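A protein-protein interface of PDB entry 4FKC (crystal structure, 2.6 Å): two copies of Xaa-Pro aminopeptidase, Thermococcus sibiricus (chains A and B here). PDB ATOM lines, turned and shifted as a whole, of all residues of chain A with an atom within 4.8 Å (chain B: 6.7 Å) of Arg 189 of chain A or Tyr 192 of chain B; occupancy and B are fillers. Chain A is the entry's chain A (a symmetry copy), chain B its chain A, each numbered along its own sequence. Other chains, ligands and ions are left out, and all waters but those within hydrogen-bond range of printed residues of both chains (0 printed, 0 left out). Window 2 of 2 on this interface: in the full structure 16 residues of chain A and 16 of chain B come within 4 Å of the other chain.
The side-chain amide oxygen (OD1) of Asn 188 of chain B sits close to the backbone carbonyl oxygen (O) of Tyr 192 of chain A (3.3 Å).
OD1 of Asn 188 of chain A sits close to O of Tyr 192 of chain B (3.3 Å).
OE2 of Glu 191 of chain A lies within salt-bridge range of NZ of Lys 195 of chain B (2.6 Å).
ND2 of Asn 196 of chain B sits at hydrogen-bond distance from OD1 of Asn 188 of chain A (3.2 Å).
The side-chain amino group (NZ) of Lys 195 of chain B is in salt-bridge range of the side-chain carboxylate (OE1) of Glu 191 of chain B (3.0 Å).
O of Lys 177 of chain A is in hydrogen-bond range of NH1 of Arg 189 of chain A, 3.4 Å away.
Among the printed residues, pairs that only touch across the chains: Asn 188 of chain A with Lys 195 of chain B, Arg 189 of chain A with Tyr 192 of chain B, Glu 191 of chain A with Glu 191 of chain B and Tyr 192 of chain A with Arg 189 of chain B.
Of chain B, only Tyr 192 (3.9 Å) comes within 4 Å of Arg 189 of chain A.
Of the printed residues of chain A, Tyr 192 of chain B touches Asn 188 (3.0 Å) and Arg 189 (3.9 Å).
Printed residues of chain A within 4 Å of Asn 196 of chain B: Asn 188.
Printed residues of chain B within 4 Å of Asn 188 of chain A: Tyr 192, Lys 195 and Asn 196.
Printed residues of chain A within 4 Å of Arg 189 of chain B: Tyr 192 (3.9 Å).
Of the printed residues of chain A, Lys 195 of chain B touches Asn 188 (3.6 Å) and Glu 191 (2.6 Å).
Printed residues of chain B within 4 Å of Glu 191 of chain A: Glu 191 and Lys 195.
Glu 185 of chain A touches none of the printed residues of chain B.
Ile 194 of chain B touches none of the printed residues of chain A.
The nearest printed residue of chain A that does not touch Tyr 192 of chain B is Tyr 192 of chain A (4.003 Å).
Of the 12 printed residues of chain A, 4 touch a printed residue of chain B.
Printed residues of chain A that touch a printed residue of chain B: Asn 188, Arg 189, Glu 191 and Tyr 192.
Hydrophobic or aromatic side chains of chain A that line the printed part of chain B: Tyr 192.
Along chain A the printed residues that touch a printed residue of chain B span positions 188 to 192.
Of the 13 printed residues of chain B, 6 touch a printed residue of chain A.
Among the printed residues, 8 pairs touch across the chains.
Asn 188 of chain A touches Tyr 192 of chain B, and with the chains exchanged Tyr 192 of chain A touches Asn 188 of chain B.
Arg 189 of chain A touches Tyr 192 of chain B, and with the chains exchanged Tyr 192 of chain A touches Arg 189 of chain B.
Glu 191 of chain B touches its own counterpart, Glu 191 of chain A.
Positions printed for both chains: 187, 188, 189, 190, 191, 192 and 193.
Of the 8 pairs that touch across the chains among the printed residues, 5 have their exchanged pair printed and touching as well.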
ATOM      1  N   PHE A 173       8.204 -10.975 -14.093  1.00  0.00           N
ATOM      2  CA  PHE A 173       7.071 -11.100 -13.198  1.00  0.00           C
ATOM      3  C   PHE A 173       5.744 -11.247 -13.939  1.00  0.00           C
ATOM      4  O   PHE A 173       4.868 -11.983 -13.492  1.00  0.00           O
ATOM      5  CB  PHE A 173       7.045  -9.924 -12.226  1.00  0.00           C
ATOM      6  CG  PHE A 173       5.788  -9.806 -11.445  1.00  0.00           C
ATOM      7  CD1 PHE A 173       4.947  -8.717 -11.642  1.00  0.00           C
ATOM      8  CD2 PHE A 173       5.440 -10.768 -10.496  1.00  0.00           C
ATOM      9  CE1 PHE A 173       3.781  -8.583 -10.914  1.00  0.00           C
ATOM     10  CE2 PHE A 173       4.272 -10.641  -9.760  1.00  0.00           C
ATOM     11  CZ  PHE A 173       3.436  -9.541  -9.975  1.00  0.00           C
ATOM     12  N   GLY A 176       4.460 -15.038 -15.301  1.00  0.00           N
ATOM     13  CA  GLY A 176       3.816 -16.056 -14.464  1.00  0.00           C
ATOM     14  C   GLY A 176       2.319 -15.808 -14.290  1.00  0.00           C
ATOM     15  O   GLY A 176       1.793 -14.806 -14.782  1.00  0.00           O
ATOM     16  N   LYS A 177       1.631 -16.716 -13.593  1.00  0.00           N
ATOM     17  CA  LYS A 177       0.199 -16.535 -13.284  1.00  0.00           C
ATOM     18  C   LYS A 177      -0.058 -15.668 -12.040  1.00  0.00           C
ATOM     19  O   LYS A 177       0.486 -15.921 -10.963  1.00  0.00           O
ATOM     20  CB  LYS A 177      -0.534 -17.888 -13.166  1.00  0.00           C
ATOM     21  CG  LYS A 177      -1.632 -18.144 -14.239  1.00  0.00           C
ATOM     22  CD  LYS A 177      -1.054 -18.428 -15.650  1.00  0.00           C
ATOM     23  CE  LYS A 177      -0.539 -19.875 -15.800  1.00  0.00           C
ATOM     24  NZ  LYS A 177       0.456 -19.977 -16.904  1.00  0.00           N
ATOM     25  N   GLU A 185       0.949 -12.247  -1.437  1.00  0.00           N
ATOM     26  CA  GLU A 185       1.810 -13.297  -2.003  1.00  0.00           C
ATOM     27  C   GLU A 185       2.612 -12.771  -3.191  1.00  0.00           C
ATOM     28  O   GLU A 185       3.776 -13.145  -3.376  1.00  0.00           O
ATOM     29  CB  GLU A 185       0.990 -14.531  -2.420  1.00  0.00           C
ATOM     30  CG  GLU A 185       0.248 -15.207  -1.256  1.00  0.00           C
ATOM     31  CD  GLU A 185      -0.921 -16.107  -1.679  1.00  0.00           C
ATOM     32  OE1 GLU A 185      -1.193 -17.086  -0.939  1.00  0.00           O
ATOM     33  OE2 GLU A 185      -1.570 -15.843  -2.728  1.00  0.00           O
ATOM     34  N   LEU A 186       1.956 -11.913  -3.982  1.00  0.00           N
ATOM     35  CA  LEU A 186       2.507 -11.300  -5.179  1.00  0.00           C
ATOM     36  C   LEU A 186       3.609 -10.318  -4.815  1.00  0.00           C
ATOM     37  O   LEU A 186       4.700 -10.362  -5.397  1.00  0.00           O
ATOM     38  CB  LEU A 186       1.397 -10.600  -5.962  1.00  0.00           C
ATOM     39  CG  LEU A 186       0.840 -11.249  -7.227  1.00  0.00           C
ATOM     40  CD1 LEU A 186       0.975 -12.751  -7.262  1.00  0.00           C
ATOM     41  CD2 LEU A 186      -0.588 -10.857  -7.393  1.00  0.00           C
ATOM     42  N   ALA A 187       3.304  -9.445  -3.852  1.00  0.00           N
ATOM     43  CA  ALA A 187       4.261  -8.496  -3.287  1.00  0.00           C
ATOM     44  C   ALA A 187       5.499  -9.225  -2.801  1.00  0.00           C
ATOM     45  O   ALA A 187       6.609  -8.702  -2.865  1.00  0.00           O
ATOM     46  CB  ALA A 187       3.636  -7.717  -2.146  1.00  0.00           C
ATOM     47  N   ASN A 188       5.310 -10.448  -2.340  1.00  0.00           N
ATOM     48  CA  ASN A 188       6.416 -11.201  -1.789  1.00  0.00           C
ATOM     49  C   ASN A 188       7.210 -11.913  -2.888  1.00  0.00           C
ATOM     50  O   ASN A 188       8.428 -12.065  -2.776  1.00  0.00           O
ATOM     51  CB  ASN A 188       5.914 -12.147  -0.693  1.00  0.00           C
ATOM     52  CG  ASN A 188       7.028 -12.963  -0.057  1.00  0.00           C
ATOM     53  OD1 ASN A 188       6.845 -14.154   0.208  1.00  0.00           O
ATOM     54  ND2 ASN A 188       8.191 -12.333   0.191  1.00  0.00           N
ATOM     55  N   ARG A 189       6.518 -12.323  -3.956  1.00  0.00           N
ATOM     56  CA  ARG A 189       7.184 -12.773  -5.181  1.00  0.00           C
ATOM     57  C   ARG A 189       8.069 -11.668  -5.782  1.00  0.00           C
ATOM     58  O   ARG A 189       9.212 -11.923  -6.139  1.00  0.00           O
ATOM     59  CB  ARG A 189       6.177 -13.290  -6.222  1.00  0.00           C
ATOM     60  CG  ARG A 189       6.125 -14.843  -6.334  1.00  0.00           C
ATOM     61  CD  ARG A 189       5.111 -15.335  -7.396  1.00  0.00           C
ATOM     62  NE  ARG A 189       5.528 -14.904  -8.737  1.00  0.00           N
ATOM     63  CZ  ARG A 189       4.844 -15.121  -9.865  1.00  0.00           C
ATOM     64  NH1 ARG A 189       3.677 -15.773  -9.840  1.00  0.00           N
ATOM     65  NH2 ARG A 189       5.331 -14.674 -11.026  1.00  0.00           N
ATOM     66  N   ILE A 190       7.538 -10.448  -5.881  1.00  0.00           N
ATOM     67  CA  ILE A 190       8.332  -9.320  -6.320  1.00  0.00           C
ATOM     68  C   ILE A 190       9.549  -9.177  -5.420  1.00  0.00           C
ATOM     69  O   ILE A 190      10.662  -9.247  -5.930  1.00  0.00           O
ATOM     70  CB  ILE A 190       7.521  -8.014  -6.447  1.00  0.00           C
ATOM     71  CG1 ILE A 190       6.538  -8.122  -7.620  1.00  0.00           C
ATOM     72  CG2 ILE A 190       8.433  -6.795  -6.652  1.00  0.00           C
ATOM     73  CD1 ILE A 190       5.381  -7.139  -7.526  1.00  0.00           C
ATOM     74  N   GLU A 191       9.362  -9.026  -4.101  1.00  0.00           N
ATOM     75  CA  GLU A 191      10.520  -8.843  -3.201  1.00  0.00           C
ATOM     76  C   GLU A 191      11.585  -9.868  -3.479  1.00  0.00           C
ATOM     77  O   GLU A 191      12.742  -9.508  -3.709  1.00  0.00           O
ATOM     78  CB  GLU A 191      10.167  -8.846  -1.708  1.00  0.00           C
ATOM     79  CG  GLU A 191      11.424  -8.883  -0.778  1.00  0.00           C
ATOM     80  CD  GLU A 191      11.266  -8.153   0.576  1.00  0.00           C
ATOM     81  OE1 GLU A 191      12.288  -7.673   1.129  1.00  0.00           O
ATOM     82  OE2 GLU A 191      10.144  -8.062   1.104  1.00  0.00           O
ATOM     83  N   TYR A 192      11.184 -11.136  -3.485  1.00  0.00           N
ATOM     84  CA  TYR A 192      12.091 -12.214  -3.772  1.00  0.00           C
ATOM     85  C   TYR A 192      12.831 -11.928  -5.062  1.00  0.00           C
ATOM     86  O   TYR A 192      14.052 -11.933  -5.072  1.00  0.00           O
ATOM     87  CB  TYR A 192      11.349 -13.548  -3.873  1.00  0.00           C
ATOM     88  CG  TYR A 192      12.251 -14.737  -4.167  1.00  0.00           C
ATOM     89  CD1 TYR A 192      13.008 -15.312  -3.158  1.00  0.00           C
ATOM     90  CD2 TYR A 192      12.333 -15.292  -5.447  1.00  0.00           C
ATOM     91  CE1 TYR A 192      13.824 -16.397  -3.396  1.00  0.00           C
ATOM     92  CE2 TYR A 192      13.170 -16.398  -5.710  1.00  0.00           C
ATOM     93  CZ  TYR A 192      13.916 -16.945  -4.666  1.00  0.00           C
ATOM     94  OH  TYR A 192      14.762 -18.030  -4.853  1.00  0.00           O
ATOM     95  N   MET A 193      12.089 -11.644  -6.135  1.00  0.00           N
ATOM     96  CA  MET A 193      12.661 -11.484  -7.474  1.00  0.00           C
ATOM     97  C   MET A 193      13.677 -10.374  -7.574  1.00  0.00           C
ATOM     98  O   MET A 193      14.682 -10.527  -8.245  1.00  0.00           O
ATOM     99  CB  MET A 193      11.570 -11.304  -8.532  1.00  0.00           C
ATOM    100  CG  MET A 193      11.073 -12.610  -9.076  1.00  0.00           C
ATOM    101  SD  MET A 193       9.831 -12.449 -10.361  1.00  0.00           S
ATOM    102  CE  MET A 193       8.650 -11.440  -9.504  1.00  0.00           C
ATOM    103  N   ALA B 187      19.256 -17.213   2.228  1.00  0.00           N
ATOM    104  CA  ALA B 187      18.688 -16.215   3.131  1.00  0.00           C
ATOM    105  C   ALA B 187      17.421 -15.629   2.537  1.00  0.00           C
ATOM    106  O   ALA B 187      16.484 -15.285   3.253  1.00  0.00           O
ATOM    107  CB  ALA B 187      19.689 -15.110   3.409  1.00  0.00           C
ATOM    108  N   ASN B 188      17.383 -15.542   1.220  1.00  0.00           N
ATOM    109  CA  ASN B 188      16.248 -14.934   0.559  1.00  0.00           C
ATOM    110  C   ASN B 188      15.110 -15.941   0.363  1.00  0.00           C
ATOM    111  O   ASN B 188      13.937 -15.571   0.416  1.00  0.00           O
ATOM    112  CB  ASN B 188      16.695 -14.263  -0.744  1.00  0.00           C
ATOM    113  CG  ASN B 188      15.553 -13.588  -1.487  1.00  0.00           C
ATOM    114  OD1 ASN B 188      15.480 -13.676  -2.715  1.00  0.00           O
ATOM    115  ND2 ASN B 188      14.650 -12.913  -0.751  1.00  0.00           N
ATOM    116  N   ARG B 189      15.467 -17.214   0.162  1.00  0.00           N
ATOM    117  CA  ARG B 189      14.493 -18.307   0.225  1.00  0.00           C
ATOM    118  C   ARG B 189      13.813 -18.380   1.603  1.00  0.00           C
ATOM    119  O   ARG B 189      12.597 -18.494   1.682  1.00  0.00           O
ATOM    120  CB  ARG B 189      15.126 -19.659  -0.143  1.00  0.00           C
ATOM    121  CG  ARG B 189      14.769 -20.156  -1.575  1.00  0.00           C
ATOM    122  CD  ARG B 189      15.411 -21.523  -1.915  1.00  0.00           C
ATOM    123  NE  ARG B 189      14.870 -22.572  -1.039  1.00  0.00           N
ATOM    124  CZ  ARG B 189      15.256 -23.851  -1.040  1.00  0.00           C
ATOM    125  NH1 ARG B 189      16.207 -24.278  -1.877  1.00  0.00           N
ATOM    126  NH2 ARG B 189      14.687 -24.710  -0.189  1.00  0.00           N
ATOM    127  N   ILE B 190      14.602 -18.308   2.676  1.00  0.00           N
ATOM    128  CA  ILE B 190      14.046 -18.247   4.011  1.00  0.00           C
ATOM    129  C   ILE B 190      13.094 -17.066   4.109  1.00  0.00           C
ATOM    130  O   ILE B 190      11.923 -17.285   4.401  1.00  0.00           O
ATOM    131  CB  ILE B 190      15.117 -18.250   5.121  1.00  0.00           C
ATOM    132  CG1 ILE B 190      15.805 -19.619   5.180  1.00  0.00           C
ATOM    133  CG2 ILE B 190      14.515 -17.918   6.495  1.00  0.00           C
ATOM    134  CD1 ILE B 190      17.167 -19.579   5.858  1.00  0.00           C
ATOM    135  N   GLU B 191      13.556 -15.839   3.828  1.00  0.00           N
ATOM    136  CA  GLU B 191      12.669 -14.664   3.952  1.00  0.00           C
ATOM    137  C   GLU B 191      11.350 -14.909   3.273  1.00  0.00           C
ATOM    138  O   GLU B 191      10.296 -14.750   3.894  1.00  0.00           O
ATOM    139  CB  GLU B 191      13.283 -13.352   3.445  1.00  0.00           C
ATOM    140  CG  GLU B 191      12.254 -12.177   3.373  1.00  0.00           C
ATOM    141  CD  GLU B 191      12.839 -10.769   3.631  1.00  0.00           C
ATOM    142  OE1 GLU B 191      12.091  -9.879   4.109  1.00  0.00           O
ATOM    143  OE2 GLU B 191      14.027 -10.531   3.351  1.00  0.00           O
ATOM    144  N   TYR B 192      11.415 -15.323   2.011  1.00  0.00           N
ATOM    145  CA  TYR B 192      10.232 -15.630   1.254  1.00  0.00           C
ATOM    146  C   TYR B 192       9.358 -16.586   2.039  1.00  0.00           C
ATOM    147  O   TYR B 192       8.194 -16.294   2.266  1.00  0.00           O
ATOM    148  CB  TYR B 192      10.587 -16.235  -0.106  1.00  0.00           C
ATOM    149  CG  TYR B 192       9.378 -16.576  -0.965  1.00  0.00           C
ATOM    150  CD1 TYR B 192       8.705 -15.582  -1.659  1.00  0.00           C
ATOM    151  CD2 TYR B 192       8.923 -17.891  -1.095  1.00  0.00           C
ATOM    152  CE1 TYR B 192       7.616 -15.868  -2.453  1.00  0.00           C
ATOM    153  CE2 TYR B 192       7.803 -18.199  -1.897  1.00  0.00           C
ATOM    154  CZ  TYR B 192       7.154 -17.169  -2.576  1.00  0.00           C
ATOM    155  OH  TYR B 192       6.045 -17.398  -3.381  1.00  0.00           O
ATOM    156  N   MET B 193       9.932 -17.708   2.481  1.00  0.00           N
ATOM    157  CA  MET B 193       9.178 -18.781   3.132  1.00  0.00           C
ATOM    158  C   MET B 193       8.470 -18.351   4.392  1.00  0.00           C
ATOM    159  O   MET B 193       7.350 -18.769   4.633  1.00  0.00           O
ATOM    160  CB  MET B 193      10.062 -20.001   3.407  1.00  0.00           C
ATOM    161  CG  MET B 193      10.107 -20.952   2.249  1.00  0.00           C
ATOM    162  SD  MET B 193      11.088 -22.426   2.544  1.00  0.00           S
ATOM    163  CE  MET B 193      12.621 -21.670   3.017  1.00  0.00           C
ATOM    164  N   ILE B 194       9.130 -17.527   5.196  1.00  0.00           N
ATOM    165  CA  ILE B 194       8.492 -16.928   6.360  1.00  0.00           C
ATOM    166  C   ILE B 194       7.226 -16.181   5.923  1.00  0.00           C
ATOM    167  O   ILE B 194       6.159 -16.374   6.493  1.00  0.00           O
ATOM    168  CB  ILE B 194       9.440 -15.968   7.106  1.00  0.00           C
ATOM    169  CG1 ILE B 194      10.679 -16.713   7.623  1.00  0.00           C
ATOM    170  CG2 ILE B 194       8.706 -15.259   8.239  1.00  0.00           C
ATOM    171  CD1 ILE B 194      11.846 -15.803   8.002  1.00  0.00           C
ATOM    172  N   LYS B 195       7.332 -15.372   4.876  1.00  0.00           N
ATOM    173  CA  LYS B 195       6.208 -14.538   4.481  1.00  0.00           C
ATOM    174  C   LYS B 195       5.113 -15.303   3.743  1.00  0.00           C
ATOM    175  O   LYS B 195       4.033 -14.765   3.512  1.00  0.00           O
ATOM    176  CB  LYS B 195       6.676 -13.315   3.710  1.00  0.00           C
ATOM    177  CG  LYS B 195       7.514 -12.365   4.547  1.00  0.00           C
ATOM    178  CD  LYS B 195       7.636 -11.029   3.859  1.00  0.00           C
ATOM    179  CE  LYS B 195       8.935 -10.362   4.212  1.00  0.00           C
ATOM    180  NZ  LYS B 195       9.296  -9.325   3.205  1.00  0.00           N
ATOM    181  N   ASN B 196       5.369 -16.566   3.413  1.00  0.00           N
ATOM    182  CA  ASN B 196       4.305 -17.446   2.930  1.00  0.00           C
ATOM    183  C   ASN B 196       3.716 -18.438   3.944  1.00  0.00           C
ATOM    184  O   ASN B 196       3.233 -19.513   3.573  1.00  0.00           O
ATOM    185  CB  ASN B 196       4.740 -18.150   1.663  1.00  0.00           C
ATOM    186  CG  ASN B 196       4.151 -17.509   0.435  1.00  0.00           C
ATOM    187  OD1 ASN B 196       3.462 -18.181  -0.337  1.00  0.00           O
ATOM    188  ND2 ASN B 196       4.380 -16.190   0.256  1.00  0.00           N
ATOM    189  N   GLU B 197       3.769 -18.069   5.223  1.00  0.00           N
ATOM    190  CA  GLU B 197       3.088 -18.805   6.283  1.00  0.00           C
ATOM    191  C   GLU B 197       1.964 -17.923   6.793  1.00  0.00           C
ATOM    192  O   GLU B 197       2.128 -16.705   6.887  1.00  0.00           O
ATOM    193  CB  GLU B 197       4.041 -19.163   7.417  1.00  0.00           C
ATOM    194  CG  GLU B 197       5.194 -20.114   7.036  1.00  0.00           C
ATOM    195  CD  GLU B 197       4.766 -21.555   6.755  1.00  0.00           C
ATOM    196  OE1 GLU B 197       3.650 -21.948   7.152  1.00  0.00           O
ATOM    197  OE2 GLU B 197       5.554 -22.304   6.130  1.00  0.00           O
ATOM    198  N   VAL B 203       9.312 -10.315   8.725  1.00  0.00           N
ATOM    199  CA  VAL B 203      10.460 -10.921   9.382  1.00  0.00           C
ATOM    200  C   VAL B 203      10.818 -10.110  10.624  1.00  0.00           C
ATOM    201  O   VAL B 203      10.482  -8.925  10.718  1.00  0.00           O
ATOM    202  CB  VAL B 203      11.675 -11.060   8.428  1.00  0.00           C
ATOM    203  CG1 VAL B 203      11.419 -12.159   7.391  1.00  0.00           C
ATOM    204  CG2 VAL B 203      12.014  -9.713   7.739  1.00  0.00           C
ATOM    205  N   PRO B 207      17.227 -12.728   7.337  1.00  0.00           N
ATOM    206  CA  PRO B 207      17.791 -14.036   7.642  1.00  0.00           C
ATOM    207  C   PRO B 207      19.301 -14.088   7.442  1.00  0.00           C
ATOM    208  O   PRO B 207      19.817 -13.526   6.462  1.00  0.00           O
ATOM    209  CB  PRO B 207      17.105 -14.948   6.624  1.00  0.00           C
ATOM    210  CG  PRO B 207      15.835 -14.304   6.350  1.00  0.00           C
ATOM    211  CD  PRO B 207      16.118 -12.843   6.375  1.00  0.00           C
